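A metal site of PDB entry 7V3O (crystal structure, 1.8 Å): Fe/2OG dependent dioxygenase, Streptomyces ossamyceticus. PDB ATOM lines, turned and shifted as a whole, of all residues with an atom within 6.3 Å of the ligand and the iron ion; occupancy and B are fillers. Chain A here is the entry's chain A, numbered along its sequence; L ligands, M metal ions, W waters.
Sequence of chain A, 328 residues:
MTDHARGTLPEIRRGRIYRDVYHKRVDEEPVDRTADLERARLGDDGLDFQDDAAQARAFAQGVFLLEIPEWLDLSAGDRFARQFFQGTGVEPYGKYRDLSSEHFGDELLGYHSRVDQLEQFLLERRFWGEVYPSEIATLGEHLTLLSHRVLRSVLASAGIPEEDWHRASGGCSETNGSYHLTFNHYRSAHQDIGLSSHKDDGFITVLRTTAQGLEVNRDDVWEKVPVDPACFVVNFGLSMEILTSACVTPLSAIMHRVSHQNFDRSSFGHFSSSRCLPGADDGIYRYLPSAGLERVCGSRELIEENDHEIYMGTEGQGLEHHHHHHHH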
ATOM      1  N   LEU A 118      13.071  18.726 -14.154  1.00  0.00           N
ATOM      2  CA  LEU A 118      13.901  17.524 -14.073  1.00  0.00           C
ATOM      3  C   LEU A 118      15.395  17.782 -14.306  1.00  0.00           C
ATOM      4  O   LEU A 118      15.775  18.516 -15.220  1.00  0.00           O
ATOM      5  CB  LEU A 118      13.410  16.551 -15.141  1.00  0.00           C
ATOM      6  CG  LEU A 118      14.189  15.255 -15.321  1.00  0.00           C
ATOM      7  CD1 LEU A 118      13.953  14.436 -14.053  1.00  0.00           C
ATOM      8  CD2 LEU A 118      13.645  14.531 -16.541  1.00  0.00           C
ATOM      9  N   GLN A 120      18.830  14.817 -14.446  1.00  0.00           N
ATOM     10  CA  GLN A 120      18.971  13.360 -14.521  1.00  0.00           C
ATOM     11  C   GLN A 120      20.424  12.935 -14.461  1.00  0.00           C
ATOM     12  O   GLN A 120      21.334  13.676 -14.843  1.00  0.00           O
ATOM     13  CB  GLN A 120      18.383  12.816 -15.821  1.00  0.00           C
ATOM     14  CG  GLN A 120      16.900  13.002 -16.005  1.00  0.00           C
ATOM     15  CD  GLN A 120      16.424  12.361 -17.305  1.00  0.00           C
ATOM     16  OE1 GLN A 120      16.760  12.831 -18.388  1.00  0.00           O
ATOM     17  NE2 GLN A 120      15.641  11.270 -17.204  1.00  0.00           N
ATOM     18  N   THR A 182      18.446   5.119 -14.884  1.00  0.00           N
ATOM     19  CA  THR A 182      18.358   6.573 -14.999  1.00  0.00           C
ATOM     20  C   THR A 182      17.756   7.121 -13.716  1.00  0.00           C
ATOM     21  O   THR A 182      16.713   6.631 -13.284  1.00  0.00           O
ATOM     22  CB  THR A 182      17.476   6.937 -16.196  1.00  0.00           C
ATOM     23  OG1 THR A 182      18.149   6.592 -17.401  1.00  0.00           O
ATOM     24  CG2 THR A 182      17.198   8.459 -16.222  1.00  0.00           C
ATOM     25  N   ASN A 184      16.351  10.432 -11.469  1.00  0.00           N
ATOM     26  CA  ASN A 184      15.602  11.663 -11.733  1.00  0.00           C
ATOM     27  C   ASN A 184      15.455  12.490 -10.460  1.00  0.00           C
ATOM     28  O   ASN A 184      15.048  11.963  -9.416  1.00  0.00           O
ATOM     29  CB  ASN A 184      14.196  11.371 -12.240  1.00  0.00           C
ATOM     30  CG  ASN A 184      14.177  10.660 -13.572  1.00  0.00           C
ATOM     31  OD1 ASN A 184      15.046  10.852 -14.414  1.00  0.00           O
ATOM     32  ND2 ASN A 184      13.133   9.872 -13.796  1.00  0.00           N
ATOM     33  N   TYR A 186      13.578  16.316  -9.375  1.00  0.00           N
ATOM     34  CA  TYR A 186      12.730  17.426  -9.810  1.00  0.00           C
ATOM     35  C   TYR A 186      13.030  18.634  -8.934  1.00  0.00           C
ATOM     36  O   TYR A 186      12.903  18.560  -7.719  1.00  0.00           O
ATOM     37  CB  TYR A 186      11.247  17.031  -9.742  1.00  0.00           C
ATOM     38  CG  TYR A 186      10.993  15.903 -10.722  1.00  0.00           C
ATOM     39  CD1 TYR A 186      11.243  14.574 -10.376  1.00  0.00           C
ATOM     40  CD2 TYR A 186      10.607  16.184 -12.029  1.00  0.00           C
ATOM     41  CE1 TYR A 186      11.078  13.544 -11.311  1.00  0.00           C
ATOM     42  CE2 TYR A 186      10.426  15.137 -12.974  1.00  0.00           C
ATOM     43  CZ  TYR A 186      10.666  13.826 -12.592  1.00  0.00           C
ATOM     44  OH  TYR A 186      10.490  12.816 -13.535  1.00  0.00           O
ATOM     45  N   LEU A 195       8.122  17.291 -15.785  1.00  0.00           N
ATOM     46  CA  LEU A 195       8.648  16.706 -17.000  1.00  0.00           C
ATOM     47  C   LEU A 195       7.500  16.694 -17.990  1.00  0.00           C
ATOM     48  O   LEU A 195       6.425  16.155 -17.691  1.00  0.00           O
ATOM     49  CB  LEU A 195       9.188  15.283 -16.764  1.00  0.00           C
ATOM     50  CG  LEU A 195       9.554  14.466 -18.003  1.00  0.00           C
ATOM     51  CD1 LEU A 195      10.671  15.159 -18.797  1.00  0.00           C
ATOM     52  CD2 LEU A 195       9.960  13.008 -17.580  1.00  0.00           C
ATOM     53  N   HIS A 198       5.413  13.052 -22.800  1.00  0.00           N
ATOM     54  CA  HIS A 198       6.249  12.305 -23.715  1.00  0.00           C
ATOM     55  C   HIS A 198       5.822  10.842 -23.693  1.00  0.00           C
ATOM     56  O   HIS A 198       5.049  10.394 -22.835  1.00  0.00           O
ATOM     57  CB  HIS A 198       7.731  12.425 -23.351  1.00  0.00           C
ATOM     58  CG  HIS A 198       8.064  11.767 -22.062  1.00  0.00           C
ATOM     59  ND1 HIS A 198       7.676  12.272 -20.845  1.00  0.00           N
ATOM     60  CD2 HIS A 198       8.702  10.592 -21.793  1.00  0.00           C
ATOM     61  CE1 HIS A 198       8.033  11.449 -19.886  1.00  0.00           C
ATOM     62  NE2 HIS A 198       8.670  10.434 -20.431  1.00  0.00           N
ATOM     63  N   LYS A 199       6.345  10.110 -24.658  1.00  0.00           N
ATOM     64  CA  LYS A 199       6.340   8.656 -24.694  1.00  0.00           C
ATOM     65  C   LYS A 199       7.781   8.192 -24.569  1.00  0.00           C
ATOM     66  O   LYS A 199       8.688   8.843 -25.092  1.00  0.00           O
ATOM     67  CB  LYS A 199       5.710   8.161 -26.000  1.00  0.00           C
ATOM     68  CG  LYS A 199       4.303   8.733 -26.216  1.00  0.00           C
ATOM     69  CD  LYS A 199       3.624   8.246 -27.501  1.00  0.00           C
ATOM     70  CE  LYS A 199       2.374   9.084 -27.777  1.00  0.00           C
ATOM     71  NZ  LYS A 199       1.182   8.303 -28.201  1.00  0.00           N
ATOM     72  N   ASP A 200       8.010   7.091 -23.843  1.00  0.00           N
ATOM     73  CA  ASP A 200       9.366   6.572 -23.697  1.00  0.00           C
ATOM     74  C   ASP A 200       9.835   5.971 -25.002  1.00  0.00           C
ATOM     75  O   ASP A 200       9.034   5.453 -25.792  1.00  0.00           O
ATOM     76  CB  ASP A 200       9.426   5.522 -22.580  1.00  0.00           C
ATOM     77  CG  ASP A 200       9.250   6.128 -21.209  1.00  0.00           C
ATOM     78  OD1 ASP A 200       9.387   7.374 -21.119  1.00  0.00           O
ATOM     79  OD2 ASP A 200       8.969   5.406 -20.234  1.00  0.00           O
ATOM     80  N   THR A 205       9.691   0.098 -19.705  1.00  0.00           N
ATOM     81  CA  THR A 205      10.196   0.936 -18.637  1.00  0.00           C
ATOM     82  C   THR A 205       9.716   0.384 -17.324  1.00  0.00           C
ATOM     83  O   THR A 205       8.509   0.143 -17.149  1.00  0.00           O
ATOM     84  CB  THR A 205       9.691   2.382 -18.774  1.00  0.00           C
ATOM     85  OG1 THR A 205      10.175   2.943 -19.995  1.00  0.00           O
ATOM     86  CG2 THR A 205      10.155   3.208 -17.583  1.00  0.00           C
ATOM     87  N   LEU A 207       9.602   1.649 -13.575  1.00  0.00           N
ATOM     88  CA  LEU A 207       9.783   2.926 -12.876  1.00  0.00           C
ATOM     89  C   LEU A 207       9.565   2.763 -11.381  1.00  0.00           C
ATOM     90  O   LEU A 207       8.543   2.232 -10.933  1.00  0.00           O
ATOM     91  CB  LEU A 207       8.811   3.978 -13.420  1.00  0.00           C
ATOM     92  CG  LEU A 207       8.904   5.348 -12.717  1.00  0.00           C
ATOM     93  CD1 LEU A 207      10.198   6.085 -13.128  1.00  0.00           C
ATOM     94  CD2 LEU A 207       7.694   6.172 -13.070  1.00  0.00           C
ATOM     95  N   ARG A 208      10.525   3.249 -10.599  1.00  0.00           N
ATOM     96  CA  ARG A 208      10.415   3.252  -9.143  1.00  0.00           C
ATOM     97  C   ARG A 208      10.108   4.691  -8.721  1.00  0.00           C
ATOM     98  O   ARG A 208      10.948   5.592  -8.837  1.00  0.00           O
ATOM     99  CB  ARG A 208      11.674   2.678  -8.511  1.00  0.00           C
ATOM    100  CG  ARG A 208      11.886   2.871  -7.018  1.00  0.00           C
ATOM    101  CD  ARG A 208      10.678   2.779  -6.196  1.00  0.00           C
ATOM    102  NE  ARG A 208      10.923   2.725  -4.757  1.00  0.00           N
ATOM    103  CZ  ARG A 208      10.084   2.089  -3.958  1.00  0.00           C
ATOM    104  NH1 ARG A 208       9.056   1.480  -4.518  1.00  0.00           N
ATOM    105  NH2 ARG A 208      10.287   2.028  -2.634  1.00  0.00           N
ATOM    106  N   THR A 209       8.892   4.912  -8.268  1.00  0.00           N
ATOM    107  CA  THR A 209       8.465   6.212  -7.794  1.00  0.00           C
ATOM    108  C   THR A 209       7.761   6.024  -6.460  1.00  0.00           C
ATOM    109  O   THR A 209       7.078   5.007  -6.262  1.00  0.00           O
ATOM    110  CB  THR A 209       7.533   6.913  -8.807  1.00  0.00           C
ATOM    111  OG1 THR A 209       7.181   8.188  -8.284  1.00  0.00           O
ATOM    112  CG2 THR A 209       6.266   6.110  -9.050  1.00  0.00           C
ATOM    113  N   GLY A 213       2.941  12.747  -8.553  1.00  0.00           N
ATOM    114  CA  GLY A 213       3.448  13.571  -9.629  1.00  0.00           C
ATOM    115  C   GLY A 213       3.272  12.984 -11.008  1.00  0.00           C
ATOM    116  O   GLY A 213       3.080  13.697 -11.996  1.00  0.00           O
ATOM    117  N   LEU A 214       3.397  11.660 -11.096  1.00  0.00           N
ATOM    118  CA  LEU A 214       3.269  11.015 -12.389  1.00  0.00           C
ATOM    119  C   LEU A 214       1.805  11.047 -12.832  1.00  0.00           C
ATOM    120  O   LEU A 214       0.898  10.795 -12.033  1.00  0.00           O
ATOM    121  CB  LEU A 214       3.770   9.570 -12.309  1.00  0.00           C
ATOM    122  CG  LEU A 214       3.745   8.787 -13.630  1.00  0.00           C
ATOM    123  CD1 LEU A 214       4.662   9.398 -14.670  1.00  0.00           C
ATOM    124  CD2 LEU A 214       4.168   7.346 -13.335  1.00  0.00           C
ATOM    125  N   ASN A 235       5.471   0.584 -17.998  1.00  0.00           N
ATOM    126  CA  ASN A 235       4.831   0.980 -19.247  1.00  0.00           C
ATOM    127  C   ASN A 235       5.731   0.610 -20.415  1.00  0.00           C
ATOM    128  O   ASN A 235       6.870   0.165 -20.241  1.00  0.00           O
ATOM    129  CB  ASN A 235       4.485   2.479 -19.280  1.00  0.00           C
ATOM    130  CG  ASN A 235       5.726   3.375 -19.124  1.00  0.00           C
ATOM    131  OD1 ASN A 235       6.066   3.782 -18.026  1.00  0.00           O
ATOM    132  ND2 ASN A 235       6.364   3.709 -20.234  1.00  0.00           N
ATOM    133  N   HIS A 256       2.843  10.334 -20.960  1.00  0.00           N
ATOM    134  CA  HIS A 256       2.848  10.597 -19.526  1.00  0.00           C
ATOM    135  C   HIS A 256       3.753  11.798 -19.228  1.00  0.00           C
ATOM    136  O   HIS A 256       4.534  12.244 -20.066  1.00  0.00           O
ATOM    137  CB  HIS A 256       3.304   9.362 -18.721  1.00  0.00           C
ATOM    138  CG  HIS A 256       4.621   8.816 -19.143  1.00  0.00           C
ATOM    139  ND1 HIS A 256       4.814   8.197 -20.355  1.00  0.00           N
ATOM    140  CD2 HIS A 256       5.824   8.829 -18.524  1.00  0.00           C
ATOM    141  CE1 HIS A 256       6.084   7.844 -20.468  1.00  0.00           C
ATOM    142  NE2 HIS A 256       6.711   8.209 -19.355  1.00  0.00           N
ATOM    143  N   ARG A 257       3.601  12.337 -18.027  1.00  0.00           N
ATOM    144  CA  ARG A 257       4.292  13.559 -17.645  1.00  0.00           C
ATOM    145  C   ARG A 257       4.421  13.572 -16.130  1.00  0.00           C
ATOM    146  O   ARG A 257       3.803  12.755 -15.440  1.00  0.00           O
ATOM    147  CB  ARG A 257       3.514  14.806 -18.145  1.00  0.00           C
ATOM    148  CG  ARG A 257       2.194  15.007 -17.405  1.00  0.00           C
ATOM    149  CD  ARG A 257       1.356  16.160 -17.992  1.00  0.00           C
ATOM    150  NE  ARG A 257       0.075  16.282 -17.321  1.00  0.00           N
ATOM    151  CZ  ARG A 257      -0.970  16.970 -17.794  1.00  0.00           C
ATOM    152  NH1 ARG A 257      -0.892  17.603 -18.954  1.00  0.00           N
ATOM    153  NH2 ARG A 257      -2.103  17.012 -17.087  1.00  0.00           N
ATOM    154  N   VAL A 258       5.180  14.530 -15.603  1.00  0.00           N
ATOM    155  CA  VAL A 258       5.257  14.745 -14.162  1.00  0.00           C
ATOM    156  C   VAL A 258       4.828  16.187 -13.922  1.00  0.00           C
ATOM    157  O   VAL A 258       5.400  17.095 -14.528  1.00  0.00           O
ATOM    158  CB  VAL A 258       6.661  14.499 -13.603  1.00  0.00           C
ATOM    159  CG1 VAL A 258       6.746  14.903 -12.136  1.00  0.00           C
ATOM    160  CG2 VAL A 258       7.068  12.998 -13.782  1.00  0.00           C
ATOM    161  N   ARG A 265      11.201  16.151  -5.594  1.00  0.00           N
ATOM    162  CA  ARG A 265      10.739  14.794  -5.839  1.00  0.00           C
ATOM    163  C   ARG A 265      11.892  14.080  -6.516  1.00  0.00           C
ATOM    164  O   ARG A 265      12.681  14.697  -7.246  1.00  0.00           O
ATOM    165  CB  ARG A 265       9.472  14.799  -6.702  1.00  0.00           C
ATOM    166  CG  ARG A 265       8.900  13.406  -7.134  1.00  0.00           C
ATOM    167  CD  ARG A 265       7.742  13.595  -8.117  1.00  0.00           C
ATOM    168  NE  ARG A 265       7.123  12.339  -8.544  1.00  0.00           N
ATOM    169  CZ  ARG A 265       7.528  11.596  -9.582  1.00  0.00           C
ATOM    170  NH1 ARG A 265       8.546  11.990 -10.301  1.00  0.00           N
ATOM    171  NH2 ARG A 265       6.892  10.453  -9.896  1.00  0.00           N
ATOM    172  N   SER A 266      11.989  12.767  -6.297  1.00  0.00           N
ATOM    173  CA  SER A 266      12.972  11.994  -7.039  1.00  0.00           C
ATOM    174  C   SER A 266      12.375  10.639  -7.363  1.00  0.00           C
ATOM    175  O   SER A 266      11.381  10.205  -6.765  1.00  0.00           O
ATOM    176  CB  SER A 266      14.296  11.846  -6.269  1.00  0.00           C
ATOM    177  OG  SER A 266      14.118  11.065  -5.080  1.00  0.00           O
ATOM    178  N   SER A 267      12.999   9.979  -8.340  1.00  0.00           N
ATOM    179  CA  SER A 267      12.554   8.678  -8.826  1.00  0.00           C
ATOM    180  C   SER A 267      13.708   8.068  -9.610  1.00  0.00           C
ATOM    181  O   SER A 267      14.712   8.716  -9.881  1.00  0.00           O
ATOM    182  CB  SER A 267      11.302   8.786  -9.704  1.00  0.00           C
ATOM    183  OG  SER A 267      11.583   9.533 -10.892  1.00  0.00           O
ATOM    184  N   PHE A 268      13.558   6.795  -9.990  1.00  0.00           N
ATOM    185  CA  PHE A 268      14.506   6.252 -10.943  1.00  0.00           C
ATOM    186  C   PHE A 268      13.830   5.160 -11.748  1.00  0.00           C
ATOM    187  O   PHE A 268      12.794   4.617 -11.340  1.00  0.00           O
ATOM    188  CB  PHE A 268      15.800   5.725 -10.272  1.00  0.00           C
ATOM    189  CG  PHE A 268      15.620   4.545  -9.359  1.00  0.00           C
ATOM    190  CD1 PHE A 268      15.734   3.244  -9.845  1.00  0.00           C
ATOM    191  CD2 PHE A 268      15.400   4.740  -8.002  1.00  0.00           C
ATOM    192  CE1 PHE A 268      15.592   2.154  -8.978  1.00  0.00           C
ATOM    193  CE2 PHE A 268      15.280   3.651  -7.110  1.00  0.00           C
ATOM    194  CZ  PHE A 268      15.361   2.347  -7.612  1.00  0.00           C
ATOM    195  N   PHE A 271      15.249   1.293 -18.248  1.00  0.00           N
ATOM    196  CA  PHE A 271      14.710   1.479 -19.596  1.00  0.00           C
ATOM    197  C   PHE A 271      15.370   0.483 -20.545  1.00  0.00           C
ATOM    198  O   PHE A 271      16.593   0.471 -20.656  1.00  0.00           O
ATOM    199  CB  PHE A 271      14.952   2.912 -20.075  1.00  0.00           C
ATOM    200  CG  PHE A 271      14.274   3.991 -19.227  1.00  0.00           C
ATOM    201  CD1 PHE A 271      14.766   4.311 -17.963  1.00  0.00           C
ATOM    202  CD2 PHE A 271      13.167   4.663 -19.709  1.00  0.00           C
ATOM    203  CE1 PHE A 271      14.136   5.330 -17.181  1.00  0.00           C
ATOM    204  CE2 PHE A 271      12.530   5.654 -18.951  1.00  0.00           C
ATOM    205  CZ  PHE A 271      13.011   5.984 -17.686  1.00  0.00           C
HETATM  206  C1  LIG L   1      11.095   9.264 -17.546  1.00  0.00           C
HETATM  207  O1  LIG L   1      11.010   9.004 -18.778  1.00  0.00           O
HETATM  208  O2  LIG L   1      12.219   9.342 -16.994  1.00  0.00           O
HETATM  209  C2  LIG L   1       9.902   9.508 -16.739  1.00  0.00           C
HETATM  210  O3  LIG L   1       8.780   9.525 -17.238  1.00  0.00           O
HETATM  211  C3  LIG L   1      10.035   9.806 -15.259  1.00  0.00           C
HETATM  212  C4  LIG L   1       8.699   9.681 -14.527  1.00  0.00           C
HETATM  213  C5  LIG L   1       8.837   9.962 -13.046  1.00  0.00           C
HETATM  214  O4  LIG L   1       7.911   9.575 -12.307  1.00  0.00           O
HETATM  215  O5  LIG L   1       9.849  10.548 -12.575  1.00  0.00           O
HETATM  216 FE    FE M   1       8.884   8.559 -19.216  1.00  0.00          FE
HETATM  217  O   HOH W   1      14.332   9.171 -18.716  1.00  0.00           O
HETATM  218  O   HOH W   2      12.130   9.034 -21.261  1.00  0.00           O
HETATM  219  O   HOH W   3       9.054   6.643 -17.996  1.00  0.00           O
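ND2 of Asn 184 is in hydrogen-bond range of O2 of the ligand (3.4 Å).
An oxygen (O4) of the ligand is in salt-bridge range of the guanidinium group (NH2) of Arg 265 (2.8 Å).
OH of Tyr 186 lies within hydrogen-bond range of O5 of the ligand.
O5 of the ligand lies within hydrogen-bond range of OG of Ser 267, at 2.6 Å.
NE2 of Gln 120 touches O2 of the ligand, at 3.9 Å.
CD2 of Leu 195 touches C2 of the ligand, 3.6 Å away.
Leu 207 touches the ligand (CD2 to O4, 3.5 Å).
CG2 of Val 258 touches C5 of the ligand, at 3.6 Å.
Phe 271 touches the ligand (CZ to O2, 3.5 Å).
Hydrophobic or aromatic side chains within 4 Å of the ligand: Tyr 186, Leu 195, His 198, Leu 207, His 256, Val 258 and Phe 271.
Of the 24 residues printed, 12 come within 4 Å of the ligand.
OD1 of Asn 184 lies within hydrogen-bond range of NE2 of Gln 120 (2.9 Å).
The side-chain hydroxyl (OG1) of Thr 205 is in hydrogen-bond range of the side-chain carboxylate (OD2) of Asp 200 (2.8 Å).
The backbone carbonyl oxygen of Ser 267 sits at hydrogen-bond distance from the backbone NH of Asn 184 (2.9 Å).
The backbone NH (N) of Tyr 186 is in hydrogen-bond range of the backbone carbonyl oxygen (O) of Arg 265, 2.8 Å away.
OG1 of Thr 209 sits at hydrogen-bond distance from NH2 of Arg 265 (2.8 Å).
The side-chain carboxylate (OD2) of Asp 200 is in hydrogen-bond range of the side-chain amide nitrogen (ND2) of Asn 235, 3.1 Å away.
N of Val 258 sits at hydrogen-bond distance from O of Leu 195 (2.9 Å).
The iron ion is bound by O3 of the ligand (2.2 Å), NE2 of His 256 (2.2 Å), O1 of the ligand (2.2 Å), NE2 of His 198 (2.2 Å), water W3 (2.3 Å) and OD1 of Asp 200 (2.3 Å).
Water W1 bridges O2 of the ligand (2.7 Å) and NE2 of Gln 120 (2.9 Å).
Of the 24 residues printed, 3 come within 4 Å of the iron ion.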
